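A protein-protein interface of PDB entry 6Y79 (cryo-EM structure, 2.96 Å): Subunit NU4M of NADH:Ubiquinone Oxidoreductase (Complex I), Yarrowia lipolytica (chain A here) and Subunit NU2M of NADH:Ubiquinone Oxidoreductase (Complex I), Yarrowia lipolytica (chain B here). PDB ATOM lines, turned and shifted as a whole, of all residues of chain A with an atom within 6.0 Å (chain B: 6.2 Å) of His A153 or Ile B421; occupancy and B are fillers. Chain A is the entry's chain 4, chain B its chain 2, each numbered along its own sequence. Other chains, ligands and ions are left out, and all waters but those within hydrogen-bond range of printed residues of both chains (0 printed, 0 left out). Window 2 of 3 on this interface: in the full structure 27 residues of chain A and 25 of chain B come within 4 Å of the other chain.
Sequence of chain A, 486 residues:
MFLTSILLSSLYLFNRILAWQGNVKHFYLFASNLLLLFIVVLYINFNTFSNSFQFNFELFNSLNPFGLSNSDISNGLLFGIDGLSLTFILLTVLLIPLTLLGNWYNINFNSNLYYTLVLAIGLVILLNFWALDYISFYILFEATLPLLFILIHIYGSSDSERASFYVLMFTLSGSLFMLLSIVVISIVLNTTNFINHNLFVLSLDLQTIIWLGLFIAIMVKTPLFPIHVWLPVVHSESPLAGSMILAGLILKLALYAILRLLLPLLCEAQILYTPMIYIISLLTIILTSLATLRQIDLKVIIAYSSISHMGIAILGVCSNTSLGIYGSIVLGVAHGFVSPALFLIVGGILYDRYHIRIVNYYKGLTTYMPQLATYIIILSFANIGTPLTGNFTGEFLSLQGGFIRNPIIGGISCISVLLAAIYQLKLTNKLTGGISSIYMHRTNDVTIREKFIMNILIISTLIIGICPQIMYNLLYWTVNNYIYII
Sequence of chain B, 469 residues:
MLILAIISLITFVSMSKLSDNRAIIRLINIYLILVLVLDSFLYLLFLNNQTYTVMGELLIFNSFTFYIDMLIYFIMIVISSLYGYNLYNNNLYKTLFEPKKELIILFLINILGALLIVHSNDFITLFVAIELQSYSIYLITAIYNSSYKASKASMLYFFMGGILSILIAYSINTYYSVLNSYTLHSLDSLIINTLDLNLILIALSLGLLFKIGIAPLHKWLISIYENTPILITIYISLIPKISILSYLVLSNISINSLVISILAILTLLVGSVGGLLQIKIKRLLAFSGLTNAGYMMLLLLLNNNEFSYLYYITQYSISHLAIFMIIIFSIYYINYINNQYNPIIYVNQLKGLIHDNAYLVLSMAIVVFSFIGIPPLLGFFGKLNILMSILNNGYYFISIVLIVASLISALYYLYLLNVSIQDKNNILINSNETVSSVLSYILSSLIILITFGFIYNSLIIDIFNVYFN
O of Ile B421 lies within hydrogen-bond range of NE2 of His A153 (3.2 Å).
The backbone NH (N) of Ile B354 lies within hydrogen-bond range of the backbone carbonyl oxygen (O) of Ser B420 (3.2 Å). OG of Ser B420 is in hydrogen-bond range of O of Leu B417, 3.4 Å away. O of Asn B418 lies within hydrogen-bond range of NE2 of Gln B422, at 2.6 Å. O of His A153 lies within hydrogen-bond range of OG of Ser A160 (3.4 Å). A ring nitrogen (ND1) of His A153 is in hydrogen-bond range of the side-chain hydroxyl of Ser A164 (3.4 Å).
Phe A149 touches Leu B417 (CE2 to CD1, 3.8 Å). Ile A150 touches Ile B421. OD1 of Asn B418 touches CE1 of His A153 (3.0 Å). Ile A154 touches Ile B354. Phe A165 touches Asn B418.
His A153 touches just these residues of chain B: Asn B418 (3.0 Å) and Ile B421 (3.2 Å). Ile B421 touches just these residues of chain A: Ile A150 (3.7 Å) and His A153 (3.2 Å). Of the printed residues of chain A, Asn B418 touches His A153 and Phe A165. Of the printed residues of chain B, Phe A165 touches Asn B418 (3.8 Å). Of the printed residues of chain A, Ile B354 touches Ile A154 (3.7 Å). Val B361 touches none of the printed residues of chain A. The nearest residue of chain B that does not touch His A153 is Gln B422 (4.5 Å).
Of the 14 printed residues of chain B, 4 touch a printed residue of chain A. Hydrophobic or aromatic side chains of chain B that line the printed part of chain A: Ile B354, Leu B417 and Ile B421. Among the printed residues, 6 pairs touch across the chains.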
ATOM      1  N   LEU A 148     -30.005  10.190 -13.772  1.00  0.00           N
ATOM      2  CA  LEU A 148     -30.538  10.385 -15.111  1.00  0.00           C
ATOM      3  C   LEU A 148     -30.097   9.276 -16.045  1.00  0.00           C
ATOM      4  O   LEU A 148     -30.893   8.807 -16.847  1.00  0.00           O
ATOM      5  CB  LEU A 148     -30.110  11.735 -15.670  1.00  0.00           C
ATOM      6  CG  LEU A 148     -30.671  12.977 -14.998  1.00  0.00           C
ATOM      7  CD1 LEU A 148     -29.954  14.204 -15.517  1.00  0.00           C
ATOM      8  CD2 LEU A 148     -32.154  13.060 -15.252  1.00  0.00           C
ATOM      9  N   PHE A 149     -28.844   8.834 -15.946  1.00  0.00           N
ATOM     10  CA  PHE A 149     -28.355   7.757 -16.804  1.00  0.00           C
ATOM     11  C   PHE A 149     -29.120   6.463 -16.563  1.00  0.00           C
ATOM     12  O   PHE A 149     -29.558   5.807 -17.512  1.00  0.00           O
ATOM     13  CB  PHE A 149     -26.861   7.549 -16.565  1.00  0.00           C
ATOM     14  CG  PHE A 149     -26.253   6.446 -17.376  1.00  0.00           C
ATOM     15  CD1 PHE A 149     -25.888   6.662 -18.688  1.00  0.00           C
ATOM     16  CD2 PHE A 149     -26.008   5.205 -16.819  1.00  0.00           C
ATOM     17  CE1 PHE A 149     -25.313   5.659 -19.434  1.00  0.00           C
ATOM     18  CE2 PHE A 149     -25.440   4.198 -17.564  1.00  0.00           C
ATOM     19  CZ  PHE A 149     -25.090   4.428 -18.873  1.00  0.00           C
ATOM     20  N   ILE A 150     -29.327   6.108 -15.294  1.00  0.00           N
ATOM     21  CA  ILE A 150     -30.034   4.877 -14.948  1.00  0.00           C
ATOM     22  C   ILE A 150     -31.502   4.969 -15.347  1.00  0.00           C
ATOM     23  O   ILE A 150     -32.070   4.018 -15.902  1.00  0.00           O
ATOM     24  CB  ILE A 150     -29.865   4.581 -13.445  1.00  0.00           C
ATOM     25  CG1 ILE A 150     -28.396   4.348 -13.093  1.00  0.00           C
ATOM     26  CG2 ILE A 150     -30.661   3.377 -13.030  1.00  0.00           C
ATOM     27  CD1 ILE A 150     -27.741   3.257 -13.860  1.00  0.00           C
ATOM     28  N   LEU A 151     -32.119   6.132 -15.123  1.00  0.00           N
ATOM     29  CA  LEU A 151     -33.517   6.345 -15.468  1.00  0.00           C
ATOM     30  C   LEU A 151     -33.745   6.291 -16.975  1.00  0.00           C
ATOM     31  O   LEU A 151     -34.667   5.620 -17.444  1.00  0.00           O
ATOM     32  CB  LEU A 151     -33.969   7.684 -14.893  1.00  0.00           C
ATOM     33  CG  LEU A 151     -35.439   8.072 -14.901  1.00  0.00           C
ATOM     34  CD1 LEU A 151     -35.793   8.619 -13.567  1.00  0.00           C
ATOM     35  CD2 LEU A 151     -35.666   9.138 -15.911  1.00  0.00           C
ATOM     36  N   ILE A 152     -32.922   6.999 -17.755  1.00  0.00           N
ATOM     37  CA  ILE A 152     -33.102   6.977 -19.202  1.00  0.00           C
ATOM     38  C   ILE A 152     -32.730   5.607 -19.756  1.00  0.00           C
ATOM     39  O   ILE A 152     -33.352   5.143 -20.700  1.00  0.00           O
ATOM     40  CB  ILE A 152     -32.315   8.101 -19.929  1.00  0.00           C
ATOM     41  CG1 ILE A 152     -32.583   9.498 -19.368  1.00  0.00           C
ATOM     42  CG2 ILE A 152     -32.680   8.190 -21.390  1.00  0.00           C
ATOM     43  CD1 ILE A 152     -33.995   9.847 -19.133  1.00  0.00           C
ATOM     44  N   HIS A 153     -31.777   4.898 -19.157  1.00  0.00           N
ATOM     45  CA  HIS A 153     -31.379   3.643 -19.780  1.00  0.00           C
ATOM     46  C   HIS A 153     -32.370   2.523 -19.511  1.00  0.00           C
ATOM     47  O   HIS A 153     -32.681   1.751 -20.422  1.00  0.00           O
ATOM     48  CB  HIS A 153     -29.991   3.225 -19.323  1.00  0.00           C
ATOM     49  CG  HIS A 153     -29.470   2.030 -20.051  1.00  0.00           C
ATOM     50  ND1 HIS A 153     -28.743   2.131 -21.212  1.00  0.00           N
ATOM     51  CD2 HIS A 153     -29.603   0.708 -19.801  1.00  0.00           C
ATOM     52  CE1 HIS A 153     -28.438   0.921 -21.639  1.00  0.00           C
ATOM     53  NE2 HIS A 153     -28.943   0.040 -20.797  1.00  0.00           N
ATOM     54  N   ILE A 154     -32.877   2.405 -18.282  1.00  0.00           N
ATOM     55  CA  ILE A 154     -33.783   1.299 -17.986  1.00  0.00           C
ATOM     56  C   ILE A 154     -35.163   1.544 -18.587  1.00  0.00           C
ATOM     57  O   ILE A 154     -35.762   0.643 -19.181  1.00  0.00           O
ATOM     58  CB  ILE A 154     -33.854   1.058 -16.471  1.00  0.00           C
ATOM     59  CG1 ILE A 154     -32.477   0.693 -15.937  1.00  0.00           C
ATOM     60  CG2 ILE A 154     -34.800  -0.068 -16.157  1.00  0.00           C
ATOM     61  CD1 ILE A 154     -32.452   0.455 -14.467  1.00  0.00           C
ATOM     62  N   TYR A 155     -35.672   2.764 -18.489  1.00  0.00           N
ATOM     63  CA  TYR A 155     -36.999   3.093 -18.987  1.00  0.00           C
ATOM     64  C   TYR A 155     -36.909   3.993 -20.211  1.00  0.00           C
ATOM     65  O   TYR A 155     -36.101   4.917 -20.257  1.00  0.00           O
ATOM     66  CB  TYR A 155     -37.815   3.759 -17.908  1.00  0.00           C
ATOM     67  CG  TYR A 155     -38.079   2.818 -16.782  1.00  0.00           C
ATOM     68  CD1 TYR A 155     -39.028   1.816 -16.913  1.00  0.00           C
ATOM     69  CD2 TYR A 155     -37.356   2.892 -15.607  1.00  0.00           C
ATOM     70  CE1 TYR A 155     -39.265   0.933 -15.898  1.00  0.00           C
ATOM     71  CE2 TYR A 155     -37.584   2.012 -14.581  1.00  0.00           C
ATOM     72  CZ  TYR A 155     -38.536   1.039 -14.733  1.00  0.00           C
ATOM     73  OH  TYR A 155     -38.759   0.164 -13.707  1.00  0.00           O
ATOM     74  N   GLY A 156     -37.735   3.735 -21.204  1.00  0.00           N
ATOM     75  CA  GLY A 156     -37.685   4.585 -22.383  1.00  0.00           C
ATOM     76  C   GLY A 156     -38.263   3.863 -23.584  1.00  0.00           C
ATOM     77  O   GLY A 156     -38.984   2.880 -23.439  1.00  0.00           O
ATOM     78  N   SER A 160     -33.239   4.103 -25.949  1.00  0.00           N
ATOM     79  CA  SER A 160     -32.950   4.733 -24.664  1.00  0.00           C
ATOM     80  C   SER A 160     -31.497   4.529 -24.228  1.00  0.00           C
ATOM     81  O   SER A 160     -31.023   5.238 -23.324  1.00  0.00           O
ATOM     82  CB  SER A 160     -33.959   4.235 -23.616  1.00  0.00           C
ATOM     83  OG  SER A 160     -33.918   2.840 -23.410  1.00  0.00           O
ATOM     84  N   GLU A 161     -30.770   3.627 -24.903  1.00  0.00           N
ATOM     85  CA  GLU A 161     -29.328   3.502 -24.689  1.00  0.00           C
ATOM     86  C   GLU A 161     -28.573   4.752 -25.161  1.00  0.00           C
ATOM     87  O   GLU A 161     -27.771   5.322 -24.409  1.00  0.00           O
ATOM     88  CB  GLU A 161     -28.803   2.216 -25.356  1.00  0.00           C
ATOM     89  CG  GLU A 161     -28.703   2.108 -26.917  1.00  0.00           C
ATOM     90  CD  GLU A 161     -30.056   2.143 -27.617  1.00  0.00           C
ATOM     91  OE1 GLU A 161     -30.100   2.438 -28.832  1.00  0.00           O
ATOM     92  OE2 GLU A 161     -31.074   1.863 -26.955  1.00  0.00           O
ATOM     93  N   SER A 164     -29.471   7.850 -22.978  1.00  0.00           N
ATOM     94  CA  SER A 164     -28.803   7.818 -21.680  1.00  0.00           C
ATOM     95  C   SER A 164     -27.319   8.131 -21.804  1.00  0.00           C
ATOM     96  O   SER A 164     -26.742   8.829 -20.947  1.00  0.00           O
ATOM     97  CB  SER A 164     -28.991   6.454 -21.034  1.00  0.00           C
ATOM     98  OG  SER A 164     -28.236   5.476 -21.716  1.00  0.00           O
ATOM     99  N   PHE A 165     -26.696   7.664 -22.883  1.00  0.00           N
ATOM    100  CA  PHE A 165     -25.297   7.995 -23.091  1.00  0.00           C
ATOM    101  C   PHE A 165     -25.115   9.479 -23.345  1.00  0.00           C
ATOM    102  O   PHE A 165     -24.245  10.088 -22.737  1.00  0.00           O
ATOM    103  CB  PHE A 165     -24.706   7.153 -24.209  1.00  0.00           C
ATOM    104  CG  PHE A 165     -24.080   5.904 -23.711  1.00  0.00           C
ATOM    105  CD1 PHE A 165     -22.806   5.920 -23.186  1.00  0.00           C
ATOM    106  CD2 PHE A 165     -24.786   4.721 -23.702  1.00  0.00           C
ATOM    107  CE1 PHE A 165     -22.238   4.767 -22.697  1.00  0.00           C
ATOM    108  CE2 PHE A 165     -24.225   3.572 -23.218  1.00  0.00           C
ATOM    109  CZ  PHE A 165     -22.952   3.593 -22.713  1.00  0.00           C
ATOM    110  N   LEU B 350     -21.782 -10.655 -18.098  1.00  0.00           N
ATOM    111  CA  LEU B 350     -22.527 -10.118 -16.967  1.00  0.00           C
ATOM    112  C   LEU B 350     -23.794  -9.388 -17.390  1.00  0.00           C
ATOM    113  O   LEU B 350     -24.250  -8.492 -16.678  1.00  0.00           O
ATOM    114  CB  LEU B 350     -21.614  -9.224 -16.119  1.00  0.00           C
ATOM    115  CG  LEU B 350     -20.732  -8.111 -16.698  1.00  0.00           C
ATOM    116  CD1 LEU B 350     -21.447  -6.779 -16.882  1.00  0.00           C
ATOM    117  CD2 LEU B 350     -19.546  -7.923 -15.814  1.00  0.00           C
ATOM    118  N   LYS B 351     -24.428  -9.834 -18.477  1.00  0.00           N
ATOM    119  CA  LYS B 351     -25.401  -9.021 -19.204  1.00  0.00           C
ATOM    120  C   LYS B 351     -26.719  -8.855 -18.451  1.00  0.00           C
ATOM    121  O   LYS B 351     -27.345  -7.796 -18.513  1.00  0.00           O
ATOM    122  CB  LYS B 351     -25.648  -9.637 -20.577  1.00  0.00           C
ATOM    123  CG  LYS B 351     -26.464  -8.780 -21.505  1.00  0.00           C
ATOM    124  CD  LYS B 351     -26.538  -9.384 -22.882  1.00  0.00           C
ATOM    125  CE  LYS B 351     -27.386 -10.632 -22.878  1.00  0.00           C
ATOM    126  NZ  LYS B 351     -28.788 -10.313 -22.528  1.00  0.00           N
ATOM    127  N   LEU B 353     -27.341  -8.788 -15.189  1.00  0.00           N
ATOM    128  CA  LEU B 353     -27.023  -8.754 -13.771  1.00  0.00           C
ATOM    129  C   LEU B 353     -27.996  -7.903 -12.961  1.00  0.00           C
ATOM    130  O   LEU B 353     -27.983  -7.973 -11.736  1.00  0.00           O
ATOM    131  CB  LEU B 353     -25.591  -8.259 -13.600  1.00  0.00           C
ATOM    132  CG  LEU B 353     -24.829  -8.474 -12.291  1.00  0.00           C
ATOM    133  CD1 LEU B 353     -24.741  -9.939 -11.934  1.00  0.00           C
ATOM    134  CD2 LEU B 353     -23.459  -7.834 -12.387  1.00  0.00           C
ATOM    135  N   ILE B 354     -28.837  -7.092 -13.590  1.00  0.00           N
ATOM    136  CA  ILE B 354     -29.767  -6.336 -12.766  1.00  0.00           C
ATOM    137  C   ILE B 354     -30.960  -7.206 -12.374  1.00  0.00           C
ATOM    138  O   ILE B 354     -31.606  -6.966 -11.351  1.00  0.00           O
ATOM    139  CB  ILE B 354     -30.179  -5.036 -13.479  1.00  0.00           C
ATOM    140  CG1 ILE B 354     -30.857  -4.075 -12.504  1.00  0.00           C
ATOM    141  CG2 ILE B 354     -31.014  -5.313 -14.710  1.00  0.00           C
ATOM    142  CD1 ILE B 354     -31.358  -2.831 -13.123  1.00  0.00           C
ATOM    143  N   HIS B 355     -31.246  -8.255 -13.133  1.00  0.00           N
ATOM    144  CA  HIS B 355     -32.379  -9.109 -12.834  1.00  0.00           C
ATOM    145  C   HIS B 355     -32.008 -10.267 -11.926  1.00  0.00           C
ATOM    146  O   HIS B 355     -32.901 -10.942 -11.405  1.00  0.00           O
ATOM    147  CB  HIS B 355     -32.990  -9.604 -14.141  1.00  0.00           C
ATOM    148  CG  HIS B 355     -33.437  -8.497 -15.040  1.00  0.00           C
ATOM    149  ND1 HIS B 355     -34.415  -7.600 -14.679  1.00  0.00           N
ATOM    150  CD2 HIS B 355     -33.024  -8.129 -16.273  1.00  0.00           C
ATOM    151  CE1 HIS B 355     -34.592  -6.730 -15.654  1.00  0.00           C
ATOM    152  NE2 HIS B 355     -33.761  -7.030 -16.635  1.00  0.00           N
ATOM    153  N   VAL B 361     -25.520  -4.737  -8.824  1.00  0.00           N
ATOM    154  CA  VAL B 361     -25.439  -3.714  -9.856  1.00  0.00           C
ATOM    155  C   VAL B 361     -25.436  -2.321  -9.236  1.00  0.00           C
ATOM    156  O   VAL B 361     -24.805  -1.402  -9.759  1.00  0.00           O
ATOM    157  CB  VAL B 361     -26.580  -3.926 -10.864  1.00  0.00           C
ATOM    158  CG1 VAL B 361     -26.706  -2.800 -11.829  1.00  0.00           C
ATOM    159  CG2 VAL B 361     -26.299  -5.141 -11.635  1.00  0.00           C
ATOM    160  N   LEU B 416     -19.487  -1.246 -18.937  1.00  0.00           N
ATOM    161  CA  LEU B 416     -19.824  -2.231 -17.908  1.00  0.00           C
ATOM    162  C   LEU B 416     -21.261  -2.069 -17.423  1.00  0.00           C
ATOM    163  O   LEU B 416     -22.006  -3.050 -17.290  1.00  0.00           O
ATOM    164  CB  LEU B 416     -18.869  -2.077 -16.732  1.00  0.00           C
ATOM    165  CG  LEU B 416     -17.408  -2.479 -16.846  1.00  0.00           C
ATOM    166  CD1 LEU B 416     -16.627  -1.875 -15.710  1.00  0.00           C
ATOM    167  CD2 LEU B 416     -17.301  -3.968 -16.795  1.00  0.00           C
ATOM    168  N   LEU B 417     -21.655  -0.825 -17.147  1.00  0.00           N
ATOM    169  CA  LEU B 417     -23.024  -0.516 -16.757  1.00  0.00           C
ATOM    170  C   LEU B 417     -24.009  -0.858 -17.858  1.00  0.00           C
ATOM    171  O   LEU B 417     -25.018  -1.516 -17.610  1.00  0.00           O
ATOM    172  CB  LEU B 417     -23.139   0.958 -16.416  1.00  0.00           C
ATOM    173  CG  LEU B 417     -22.836   1.337 -14.992  1.00  0.00           C
ATOM    174  CD1 LEU B 417     -23.112   2.778 -14.881  1.00  0.00           C
ATOM    175  CD2 LEU B 417     -23.738   0.562 -14.082  1.00  0.00           C
ATOM    176  N   ASN B 418     -23.715  -0.415 -19.082  1.00  0.00           N
ATOM    177  CA  ASN B 418     -24.562  -0.644 -20.246  1.00  0.00           C
ATOM    178  C   ASN B 418     -24.803  -2.126 -20.483  1.00  0.00           C
ATOM    179  O   ASN B 418     -25.897  -2.524 -20.892  1.00  0.00           O
ATOM    180  CB  ASN B 418     -23.904   0.003 -21.464  1.00  0.00           C
ATOM    181  CG  ASN B 418     -24.687  -0.181 -22.731  1.00  0.00           C
ATOM    182  OD1 ASN B 418     -25.901  -0.305 -22.719  1.00  0.00           O
ATOM    183  ND2 ASN B 418     -23.984  -0.199 -23.849  1.00  0.00           N
ATOM    184  N   VAL B 419     -23.812  -2.962 -20.185  1.00  0.00           N
ATOM    185  CA  VAL B 419     -24.032  -4.394 -20.309  1.00  0.00           C
ATOM    186  C   VAL B 419     -24.881  -4.912 -19.153  1.00  0.00           C
ATOM    187  O   VAL B 419     -25.839  -5.649 -19.374  1.00  0.00           O
ATOM    188  CB  VAL B 419     -22.687  -5.126 -20.435  1.00  0.00           C
ATOM    189  CG1 VAL B 419     -22.864  -6.582 -20.321  1.00  0.00           C
ATOM    190  CG2 VAL B 419     -22.114  -4.843 -21.781  1.00  0.00           C
ATOM    191  N   SER B 420     -24.604  -4.486 -17.919  1.00  0.00           N
ATOM    192  CA  SER B 420     -25.237  -5.156 -16.779  1.00  0.00           C
ATOM    193  C   SER B 420     -26.689  -4.724 -16.554  1.00  0.00           C
ATOM    194  O   SER B 420     -27.482  -5.502 -16.019  1.00  0.00           O
ATOM    195  CB  SER B 420     -24.416  -4.938 -15.511  1.00  0.00           C
ATOM    196  OG  SER B 420     -24.598  -3.643 -15.008  1.00  0.00           O
ATOM    197  N   ILE B 421     -27.068  -3.494 -16.905  1.00  0.00           N
ATOM    198  CA  ILE B 421     -28.491  -3.167 -16.807  1.00  0.00           C
ATOM    199  C   ILE B 421     -29.159  -3.437 -18.156  1.00  0.00           C
ATOM    200  O   ILE B 421     -29.404  -2.536 -18.962  1.00  0.00           O
ATOM    201  CB  ILE B 421     -28.750  -1.736 -16.269  1.00  0.00           C
ATOM    202  CG1 ILE B 421     -27.972  -0.622 -16.966  1.00  0.00           C
ATOM    203  CG2 ILE B 421     -28.322  -1.654 -14.857  1.00  0.00           C
ATOM    204  CD1 ILE B 421     -28.386   0.753 -16.532  1.00  0.00           C
ATOM    205  N   GLN B 422     -29.486  -4.697 -18.404  1.00  0.00           N
ATOM    206  CA  GLN B 422     -30.106  -5.093 -19.654  1.00  0.00           C
ATOM    207  C   GLN B 422     -31.045  -6.255 -19.391  1.00  0.00           C
ATOM    208  O   GLN B 422     -30.993  -6.903 -18.345  1.00  0.00           O
ATOM    209  CB  GLN B 422     -29.063  -5.472 -20.706  1.00  0.00           C
ATOM    210  CG  GLN B 422     -28.655  -4.330 -21.600  1.00  0.00           C
ATOM    211  CD  GLN B 422     -27.548  -4.709 -22.537  1.00  0.00           C
ATOM    212  OE1 GLN B 422     -27.325  -5.883 -22.799  1.00  0.00           O
ATOM    213  NE2 GLN B 422     -26.838  -3.718 -23.048  1.00  0.00           N
ATOM    214  N   ASP B 423     -31.912  -6.513 -20.359  1.00  0.00           N
ATOM    215  CA  ASP B 423     -32.859  -7.607 -20.252  1.00  0.00           C
ATOM    216  C   ASP B 423     -32.158  -8.941 -20.457  1.00  0.00           C
ATOM    217  O   ASP B 423     -31.246  -9.063 -21.277  1.00  0.00           O
ATOM    218  CB  ASP B 423     -33.981  -7.443 -21.275  1.00  0.00           C
ATOM    219  CG  ASP B 423     -34.917  -6.305 -20.933  1.00  0.00           C
ATOM    220  OD1 ASP B 423     -35.074  -6.005 -19.731  1.00  0.00           O
ATOM    221  OD2 ASP B 423     -35.502  -5.714 -21.864  1.00  0.00           O
